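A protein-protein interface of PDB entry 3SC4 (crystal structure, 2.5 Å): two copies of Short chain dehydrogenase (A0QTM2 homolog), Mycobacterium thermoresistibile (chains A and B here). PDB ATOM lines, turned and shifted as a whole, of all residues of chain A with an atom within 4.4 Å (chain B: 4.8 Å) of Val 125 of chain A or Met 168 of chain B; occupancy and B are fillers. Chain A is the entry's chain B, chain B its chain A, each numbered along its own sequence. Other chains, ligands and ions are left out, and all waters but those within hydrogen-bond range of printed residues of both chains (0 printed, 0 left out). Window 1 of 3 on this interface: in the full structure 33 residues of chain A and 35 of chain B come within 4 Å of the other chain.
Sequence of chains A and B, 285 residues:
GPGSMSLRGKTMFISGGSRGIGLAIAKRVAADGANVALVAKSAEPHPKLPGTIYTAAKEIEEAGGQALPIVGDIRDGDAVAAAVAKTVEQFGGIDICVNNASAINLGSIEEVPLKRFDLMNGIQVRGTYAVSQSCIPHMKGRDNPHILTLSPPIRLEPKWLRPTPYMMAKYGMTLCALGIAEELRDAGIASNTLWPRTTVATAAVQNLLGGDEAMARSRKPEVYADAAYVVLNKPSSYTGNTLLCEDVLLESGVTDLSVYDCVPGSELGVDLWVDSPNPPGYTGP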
ATOM      1  N   MET A 120      34.143 -26.752 -16.176  1.00  0.00           N
ATOM      2  CA  MET A 120      34.556 -25.352 -16.017  1.00  0.00           C
ATOM      3  C   MET A 120      33.580 -24.349 -16.685  1.00  0.00           C
ATOM      4  O   MET A 120      33.198 -23.347 -16.095  1.00  0.00           O
ATOM      5  CB  MET A 120      35.978 -25.148 -16.586  1.00  0.00           C
ATOM      6  CG  MET A 120      37.070 -25.867 -15.811  1.00  0.00           C
ATOM      7  SD  MET A 120      38.763 -25.340 -16.165  1.00  0.00           S
ATOM      8  CE  MET A 120      39.101 -26.597 -17.336  1.00  0.00           C
ATOM      9  N   ASN A 121      33.250 -24.609 -17.945  1.00  0.00           N
ATOM     10  CA  ASN A 121      32.333 -23.795 -18.707  1.00  0.00           C
ATOM     11  C   ASN A 121      30.974 -23.863 -18.002  1.00  0.00           C
ATOM     12  O   ASN A 121      30.318 -22.827 -17.777  1.00  0.00           O
ATOM     13  CB  ASN A 121      32.282 -24.335 -20.131  1.00  0.00           C
ATOM     14  CG  ASN A 121      31.339 -23.551 -21.069  1.00  0.00           C
ATOM     15  OD1 ASN A 121      31.671 -22.452 -21.558  1.00  0.00           O
ATOM     16  ND2 ASN A 121      30.210 -24.170 -21.402  1.00  0.00           N
ATOM     17  N   ILE A 123      29.995 -24.565 -14.793  1.00  0.00           N
ATOM     18  CA  ILE A 123      29.827 -23.918 -13.523  1.00  0.00           C
ATOM     19  C   ILE A 123      30.044 -22.406 -13.639  1.00  0.00           C
ATOM     20  O   ILE A 123      29.330 -21.631 -13.017  1.00  0.00           O
ATOM     21  CB  ILE A 123      30.778 -24.508 -12.474  1.00  0.00           C
ATOM     22  CG1 ILE A 123      30.358 -25.952 -12.155  1.00  0.00           C
ATOM     23  CG2 ILE A 123      30.727 -23.689 -11.240  1.00  0.00           C
ATOM     24  CD1 ILE A 123      31.332 -26.724 -11.244  1.00  0.00           C
ATOM     25  N   GLN A 124      31.004 -21.981 -14.438  1.00  0.00           N
ATOM     26  CA  GLN A 124      31.423 -20.579 -14.418  1.00  0.00           C
ATOM     27  C   GLN A 124      30.760 -19.678 -15.463  1.00  0.00           C
ATOM     28  O   GLN A 124      30.321 -18.565 -15.137  1.00  0.00           O
ATOM     29  CB  GLN A 124      32.962 -20.473 -14.497  1.00  0.00           C
ATOM     30  CG  GLN A 124      33.603 -20.785 -13.157  1.00  0.00           C
ATOM     31  CD  GLN A 124      35.072 -21.220 -13.193  1.00  0.00           C
ATOM     32  OE1 GLN A 124      35.832 -20.898 -12.262  1.00  0.00           O
ATOM     33  NE2 GLN A 124      35.460 -21.982 -14.216  1.00  0.00           N
ATOM     34  N   VAL A 125      30.713 -20.124 -16.710  1.00  0.00           N
ATOM     35  CA  VAL A 125      30.170 -19.293 -17.776  1.00  0.00           C
ATOM     36  C   VAL A 125      28.679 -19.503 -17.796  1.00  0.00           C
ATOM     37  O   VAL A 125      27.926 -18.580 -17.591  1.00  0.00           O
ATOM     38  CB  VAL A 125      30.745 -19.646 -19.125  1.00  0.00           C
ATOM     39  CG1 VAL A 125      30.220 -18.691 -20.168  1.00  0.00           C
ATOM     40  CG2 VAL A 125      32.288 -19.641 -19.059  1.00  0.00           C
ATOM     41  N   ARG A 126      28.261 -20.738 -17.984  1.00  0.00           N
ATOM     42  CA  ARG A 126      26.850 -21.068 -17.969  1.00  0.00           C
ATOM     43  C   ARG A 126      26.241 -20.782 -16.592  1.00  0.00           C
ATOM     44  O   ARG A 126      25.174 -20.180 -16.488  1.00  0.00           O
ATOM     45  CB  ARG A 126      26.663 -22.522 -18.360  1.00  0.00           C
ATOM     46  CG  ARG A 126      25.214 -22.890 -18.619  1.00  0.00           C
ATOM     47  CD  ARG A 126      25.086 -24.320 -19.112  1.00  0.00           C
ATOM     48  NE  ARG A 126      23.704 -24.752 -19.347  1.00  0.00           N
ATOM     49  CZ  ARG A 126      22.935 -25.384 -18.461  1.00  0.00           C
ATOM     50  NH1 ARG A 126      23.373 -25.609 -17.229  1.00  0.00           N
ATOM     51  NH2 ARG A 126      21.698 -25.778 -18.798  1.00  0.00           N
ATOM     52  N   GLY A 127      26.934 -21.193 -15.539  1.00  0.00           N
ATOM     53  CA  GLY A 127      26.453 -20.977 -14.188  1.00  0.00           C
ATOM     54  C   GLY A 127      26.260 -19.513 -13.826  1.00  0.00           C
ATOM     55  O   GLY A 127      25.229 -19.136 -13.238  1.00  0.00           O
ATOM     56  N   THR A 128      27.231 -18.671 -14.170  1.00  0.00           N
ATOM     57  CA  THR A 128      27.098 -17.242 -13.871  1.00  0.00           C
ATOM     58  C   THR A 128      25.909 -16.660 -14.622  1.00  0.00           C
ATOM     59  O   THR A 128      25.191 -15.803 -14.083  1.00  0.00           O
ATOM     60  CB  THR A 128      28.381 -16.476 -14.194  1.00  0.00           C
ATOM     61  OG1 THR A 128      29.426 -16.944 -13.323  1.00  0.00           O
ATOM     62  CG2 THR A 128      28.190 -14.957 -14.032  1.00  0.00           C
ATOM     63  N   TYR A 129      25.698 -17.141 -15.849  1.00  0.00           N
ATOM     64  CA  TYR A 129      24.579 -16.713 -16.665  1.00  0.00           C
ATOM     65  C   TYR A 129      23.249 -17.139 -15.998  1.00  0.00           C
ATOM     66  O   TYR A 129      22.379 -16.307 -15.743  1.00  0.00           O
ATOM     67  CB  TYR A 129      24.712 -17.307 -18.070  1.00  0.00           C
ATOM     68  CG  TYR A 129      23.651 -16.848 -19.050  1.00  0.00           C
ATOM     69  CD1 TYR A 129      23.808 -15.674 -19.767  1.00  0.00           C
ATOM     70  CD2 TYR A 129      22.501 -17.587 -19.265  1.00  0.00           C
ATOM     71  CE1 TYR A 129      22.853 -15.260 -20.667  1.00  0.00           C
ATOM     72  CE2 TYR A 129      21.522 -17.157 -20.157  1.00  0.00           C
ATOM     73  CZ  TYR A 129      21.719 -15.992 -20.852  1.00  0.00           C
ATOM     74  OH  TYR A 129      20.784 -15.538 -21.733  1.00  0.00           O
ATOM     75  N   MET A 168      39.287 -19.220 -20.814  1.00  0.00           N
ATOM     76  CA  MET A 168      37.968 -19.106 -21.467  1.00  0.00           C
ATOM     77  C   MET A 168      36.829 -18.995 -20.442  1.00  0.00           C
ATOM     78  O   MET A 168      35.886 -18.207 -20.615  1.00  0.00           O
ATOM     79  CB  MET A 168      37.693 -20.312 -22.392  1.00  0.00           C
ATOM     80  CG  MET A 168      38.414 -20.215 -23.694  1.00  0.00           C
ATOM     81  SD  MET A 168      38.276 -21.732 -24.645  1.00  0.00           S
ATOM     82  CE  MET A 168      36.507 -21.730 -25.007  1.00  0.00           C
ATOM     83  N   ALA A 169      36.894 -19.845 -19.429  1.00  0.00           N
ATOM     84  CA  ALA A 169      35.870 -19.905 -18.416  1.00  0.00           C
ATOM     85  C   ALA A 169      35.894 -18.621 -17.597  1.00  0.00           C
ATOM     86  O   ALA A 169      34.848 -17.986 -17.409  1.00  0.00           O
ATOM     87  CB  ALA A 169      36.046 -21.148 -17.527  1.00  0.00           C
ATOM     88  N   GLY A 172      34.944 -15.653 -19.706  1.00  0.00           N
ATOM     89  CA  GLY A 172      33.521 -15.822 -19.993  1.00  0.00           C
ATOM     90  C   GLY A 172      32.631 -15.300 -18.882  1.00  0.00           C
ATOM     91  O   GLY A 172      31.639 -14.631 -19.154  1.00  0.00           O
ATOM     92  N   MET A 173      33.012 -15.577 -17.623  1.00  0.00           N
ATOM     93  CA  MET A 173      32.323 -15.026 -16.428  1.00  0.00           C
ATOM     94  C   MET A 173      32.372 -13.519 -16.446  1.00  0.00           C
ATOM     95  O   MET A 173      31.370 -12.863 -16.232  1.00  0.00           O
ATOM     96  CB  MET A 173      32.980 -15.472 -15.114  1.00  0.00           C
ATOM     97  CG  MET A 173      32.536 -16.734 -14.562  1.00  0.00           C
ATOM     98  SD  MET A 173      33.367 -17.130 -13.007  1.00  0.00           S
ATOM     99  CE  MET A 173      32.340 -16.436 -11.718  1.00  0.00           C
ATOM    100  N   CYS A 176      30.157 -12.063 -19.135  1.00  0.00           N
ATOM    101  CA  CYS A 176      28.777 -12.115 -18.715  1.00  0.00           C
ATOM    102  C   CYS A 176      28.461 -10.906 -17.825  1.00  0.00           C
ATOM    103  O   CYS A 176      27.463 -10.200 -18.038  1.00  0.00           O
ATOM    104  CB  CYS A 176      28.507 -13.402 -17.985  1.00  0.00           C
ATOM    105  SG  CYS A 176      26.787 -13.646 -17.604  1.00  0.00           S
ATOM    106  N   PHE B 117      20.771 -20.369 -24.757  1.00  0.00           N
ATOM    107  CA  PHE B 117      22.149 -20.032 -24.430  1.00  0.00           C
ATOM    108  C   PHE B 117      23.065 -21.231 -24.695  1.00  0.00           C
ATOM    109  O   PHE B 117      24.108 -21.098 -25.340  1.00  0.00           O
ATOM    110  CB  PHE B 117      22.234 -19.581 -22.969  1.00  0.00           C
ATOM    111  CG  PHE B 117      23.614 -19.357 -22.488  1.00  0.00           C
ATOM    112  CD1 PHE B 117      24.162 -18.094 -22.505  1.00  0.00           C
ATOM    113  CD2 PHE B 117      24.372 -20.418 -22.023  1.00  0.00           C
ATOM    114  CE1 PHE B 117      25.421 -17.876 -22.079  1.00  0.00           C
ATOM    115  CE2 PHE B 117      25.657 -20.211 -21.583  1.00  0.00           C
ATOM    116  CZ  PHE B 117      26.186 -18.936 -21.614  1.00  0.00           C
ATOM    117  N   ASN B 121      26.430 -21.495 -26.787  1.00  0.00           N
ATOM    118  CA  ASN B 121      27.621 -21.848 -26.047  1.00  0.00           C
ATOM    119  C   ASN B 121      28.166 -23.173 -26.570  1.00  0.00           C
ATOM    120  O   ASN B 121      29.360 -23.285 -26.907  1.00  0.00           O
ATOM    121  CB  ASN B 121      27.316 -21.911 -24.539  1.00  0.00           C
ATOM    122  CG  ASN B 121      28.534 -22.229 -23.703  1.00  0.00           C
ATOM    123  OD1 ASN B 121      29.372 -21.376 -23.475  1.00  0.00           O
ATOM    124  ND2 ASN B 121      28.637 -23.462 -23.256  1.00  0.00           N
ATOM    125  N   VAL B 125      31.407 -22.166 -28.529  1.00  0.00           N
ATOM    126  CA  VAL B 125      32.506 -22.070 -27.577  1.00  0.00           C
ATOM    127  C   VAL B 125      32.998 -23.482 -27.325  1.00  0.00           C
ATOM    128  O   VAL B 125      34.117 -23.835 -27.670  1.00  0.00           O
ATOM    129  CB  VAL B 125      32.038 -21.428 -26.281  1.00  0.00           C
ATOM    130  CG1 VAL B 125      33.170 -21.365 -25.286  1.00  0.00           C
ATOM    131  CG2 VAL B 125      31.444 -20.058 -26.581  1.00  0.00           C
ATOM    132  N   THR B 164      24.370  -9.765 -24.648  1.00  0.00           N
ATOM    133  CA  THR B 164      25.260 -10.567 -23.851  1.00  0.00           C
ATOM    134  C   THR B 164      25.385 -12.013 -24.298  1.00  0.00           C
ATOM    135  O   THR B 164      26.480 -12.483 -24.520  1.00  0.00           O
ATOM    136  CB  THR B 164      24.878 -10.449 -22.364  1.00  0.00           C
ATOM    137  OG1 THR B 164      24.918  -9.058 -22.008  1.00  0.00           O
ATOM    138  CG2 THR B 164      25.839 -11.242 -21.493  1.00  0.00           C
ATOM    139  N   PRO B 165      24.273 -12.719 -24.472  1.00  0.00           N
ATOM    140  CA  PRO B 165      24.453 -14.123 -24.762  1.00  0.00           C
ATOM    141  C   PRO B 165      25.283 -14.398 -25.997  1.00  0.00           C
ATOM    142  O   PRO B 165      26.170 -15.255 -25.971  1.00  0.00           O
ATOM    143  CB  PRO B 165      23.022 -14.610 -24.968  1.00  0.00           C
ATOM    144  CG  PRO B 165      22.217 -13.753 -24.174  1.00  0.00           C
ATOM    145  CD  PRO B 165      22.875 -12.420 -24.142  1.00  0.00           C
ATOM    146  N   TYR B 166      24.986 -13.685 -27.074  1.00  0.00           N
ATOM    147  CA  TYR B 166      25.670 -13.900 -28.334  1.00  0.00           C
ATOM    148  C   TYR B 166      27.119 -13.409 -28.298  1.00  0.00           C
ATOM    149  O   TYR B 166      28.002 -14.039 -28.872  1.00  0.00           O
ATOM    150  CB  TYR B 166      24.903 -13.207 -29.457  1.00  0.00           C
ATOM    151  CG  TYR B 166      25.456 -13.423 -30.846  1.00  0.00           C
ATOM    152  CD1 TYR B 166      25.596 -14.693 -31.364  1.00  0.00           C
ATOM    153  CD2 TYR B 166      25.801 -12.337 -31.670  1.00  0.00           C
ATOM    154  CE1 TYR B 166      26.093 -14.898 -32.656  1.00  0.00           C
ATOM    155  CE2 TYR B 166      26.284 -12.537 -32.963  1.00  0.00           C
ATOM    156  CZ  TYR B 166      26.431 -13.827 -33.440  1.00  0.00           C
ATOM    157  OH  TYR B 166      26.896 -14.053 -34.708  1.00  0.00           O
ATOM    158  N   MET B 167      27.332 -12.259 -27.660  1.00  0.00           N
ATOM    159  CA  MET B 167      28.665 -11.722 -27.459  1.00  0.00           C
ATOM    160  C   MET B 167      29.515 -12.719 -26.660  1.00  0.00           C
ATOM    161  O   MET B 167      30.668 -12.921 -26.993  1.00  0.00           O
ATOM    162  CB  MET B 167      28.593 -10.368 -26.758  1.00  0.00           C
ATOM    163  CG  MET B 167      29.939  -9.770 -26.374  1.00  0.00           C
ATOM    164  SD  MET B 167      30.609 -10.467 -24.835  1.00  0.00           S
ATOM    165  CE  MET B 167      29.450  -9.821 -23.645  1.00  0.00           C
ATOM    166  N   MET B 168      28.954 -13.358 -25.638  1.00  0.00           N
ATOM    167  CA  MET B 168      29.712 -14.364 -24.881  1.00  0.00           C
ATOM    168  C   MET B 168      30.181 -15.478 -25.787  1.00  0.00           C
ATOM    169  O   MET B 168      31.278 -16.005 -25.642  1.00  0.00           O
ATOM    170  CB  MET B 168      28.859 -14.945 -23.760  1.00  0.00           C
ATOM    171  CG  MET B 168      28.644 -13.926 -22.630  1.00  0.00           C
ATOM    172  SD  MET B 168      27.594 -14.496 -21.326  1.00  0.00           S
ATOM    173  CE  MET B 168      28.524 -15.944 -20.812  1.00  0.00           C
ATOM    174  N   ALA B 169      29.322 -15.866 -26.711  1.00  0.00           N
ATOM    175  CA  ALA B 169      29.574 -17.035 -27.524  1.00  0.00           C
ATOM    176  C   ALA B 169      30.616 -16.686 -28.559  1.00  0.00           C
ATOM    177  O   ALA B 169      31.613 -17.413 -28.709  1.00  0.00           O
ATOM    178  CB  ALA B 169      28.258 -17.536 -28.211  1.00  0.00           C
ATOM    179  N   LYS B 170      30.404 -15.577 -29.264  1.00  0.00           N
ATOM    180  CA  LYS B 170      31.317 -15.222 -30.319  1.00  0.00           C
ATOM    181  C   LYS B 170      32.694 -14.860 -29.750  1.00  0.00           C
ATOM    182  O   LYS B 170      33.709 -15.246 -30.346  1.00  0.00           O
ATOM    183  CB  LYS B 170      30.775 -14.107 -31.211  1.00  0.00           C
ATOM    184  CG  LYS B 170      29.529 -14.494 -31.967  1.00  0.00           C
ATOM    185  CD  LYS B 170      29.614 -15.810 -32.739  1.00  0.00           C
ATOM    186  CE  LYS B 170      30.726 -15.768 -33.747  1.00  0.00           C
ATOM    187  NZ  LYS B 170      30.665 -16.900 -34.701  1.00  0.00           N
ATOM    188  N   TYR B 171      32.719 -14.111 -28.640  1.00  0.00           N
ATOM    189  CA  TYR B 171      33.968 -13.760 -27.953  1.00  0.00           C
ATOM    190  C   TYR B 171      34.626 -15.025 -27.372  1.00  0.00           C
ATOM    191  O   TYR B 171      35.832 -15.187 -27.429  1.00  0.00           O
ATOM    192  CB  TYR B 171      33.733 -12.744 -26.834  1.00  0.00           C
ATOM    193  CG  TYR B 171      33.597 -11.262 -27.233  1.00  0.00           C
ATOM    194  CD1 TYR B 171      33.218 -10.869 -28.518  1.00  0.00           C
ATOM    195  CD2 TYR B 171      33.818 -10.253 -26.286  1.00  0.00           C
ATOM    196  CE1 TYR B 171      33.080  -9.525 -28.861  1.00  0.00           C
ATOM    197  CE2 TYR B 171      33.699  -8.895 -26.626  1.00  0.00           C
ATOM    198  CZ  TYR B 171      33.326  -8.541 -27.923  1.00  0.00           C
ATOM    199  OH  TYR B 171      33.200  -7.197 -28.257  1.00  0.00           O
ATOM    200  N   GLY B 172      33.844 -15.930 -26.815  1.00  0.00           N
ATOM    201  CA  GLY B 172      34.419 -17.166 -26.318  1.00  0.00           C
ATOM    202  C   GLY B 172      35.122 -17.930 -27.435  1.00  0.00           C
ATOM    203  O   GLY B 172      36.225 -18.447 -27.265  1.00  0.00           O
ATOM    204  N   MET B 173      34.476 -17.963 -28.592  1.00  0.00           N
ATOM    205  CA  MET B 173      35.049 -18.520 -29.802  1.00  0.00           C
ATOM    206  C   MET B 173      36.408 -17.901 -30.098  1.00  0.00           C
ATOM    207  O   MET B 173      37.400 -18.610 -30.342  1.00  0.00           O
ATOM    208  CB  MET B 173      34.102 -18.252 -30.958  1.00  0.00           C
ATOM    209  CG  MET B 173      33.968 -19.352 -31.927  1.00  0.00           C
ATOM    210  SD  MET B 173      32.547 -19.152 -33.024  1.00  0.00           S
ATOM    211  CE  MET B 173      33.245 -20.057 -34.415  1.00  0.00           C
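Printed residues of chain A that touch a printed residue of chain B: Asn 121, Val 125, Arg 126, Tyr 129, Met 168, Gly 172 and Cys 176. Hydrophobic or aromatic side chains of chain B that line the printed part of chain A: Phe 117, Val 125, Pro 165 and Met 168. Among the printed residues, no Asp or Glu carboxylate lies within 4 Å of a Lys or Arg side-chain nitrogen of the other chain.
Among the printed residues, merely in contact across the chains: Val 125 of chain A with Met 168 of chain B (3.3 Å), Arg 126 of chain A with Phe 117 of chain B (3.9 Å), Tyr 129 of chain A with Phe 117 of chain B (3.6 Å), Tyr 129 of chain A with Pro 165 of chain B (3.3 Å), Met 168 of chain A with Val 125 of chain B (3.4 Å), Met 168 of chain A with Gly 172 of chain B (3.99 Å), Gly 172 of chain A with Met 168 of chain B (3.8 Å), Cys 176 of chain A with Thr 164 of chain B (3.96 Å) and Cys 176 of chain A with Met 168 of chain B (3.6 Å).
Of the printed residues of chain B, Tyr 129 of chain A touches Phe 117 and Pro 165. Printed residues of chain A within 4 Å of Phe 117 of chain B: Arg 126 and Tyr 129. Of chain A, only Val 125, Gly 172 and Cys 176 come within 4 Å of Met 168 of chain B. The nearest residue of chain A that does not touch Met 168 of chain B is Tyr 129 of chain A (4.3 Å).
The backbone NH (N) of Arg 126 of chain A lies within hydrogen-bond range of the backbone carbonyl oxygen (O) of Asn 121 of chain A (2.9 Å).
ND2 of Asn 121 of chain B lies close to ND2 of Asn 121 of chain A, at 2.5 Å.
Asn 121 of chain B touches its own counterpart, Asn 121 of chain A. Val 125 of chain A touches Met 168 of chain B, and with the chains exchanged Met 168 of chain A touches Val 125 of chain B. Met 168 of chain A touches Gly 172 of chain B, and with the chains exchanged Gly 172 of chain A touches Met 168 of chain B. 6 positions are printed for both chains. Of the 10 pairs that touch across the chains among the printed residues, 5 have their exchanged pair printed and touching as well.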
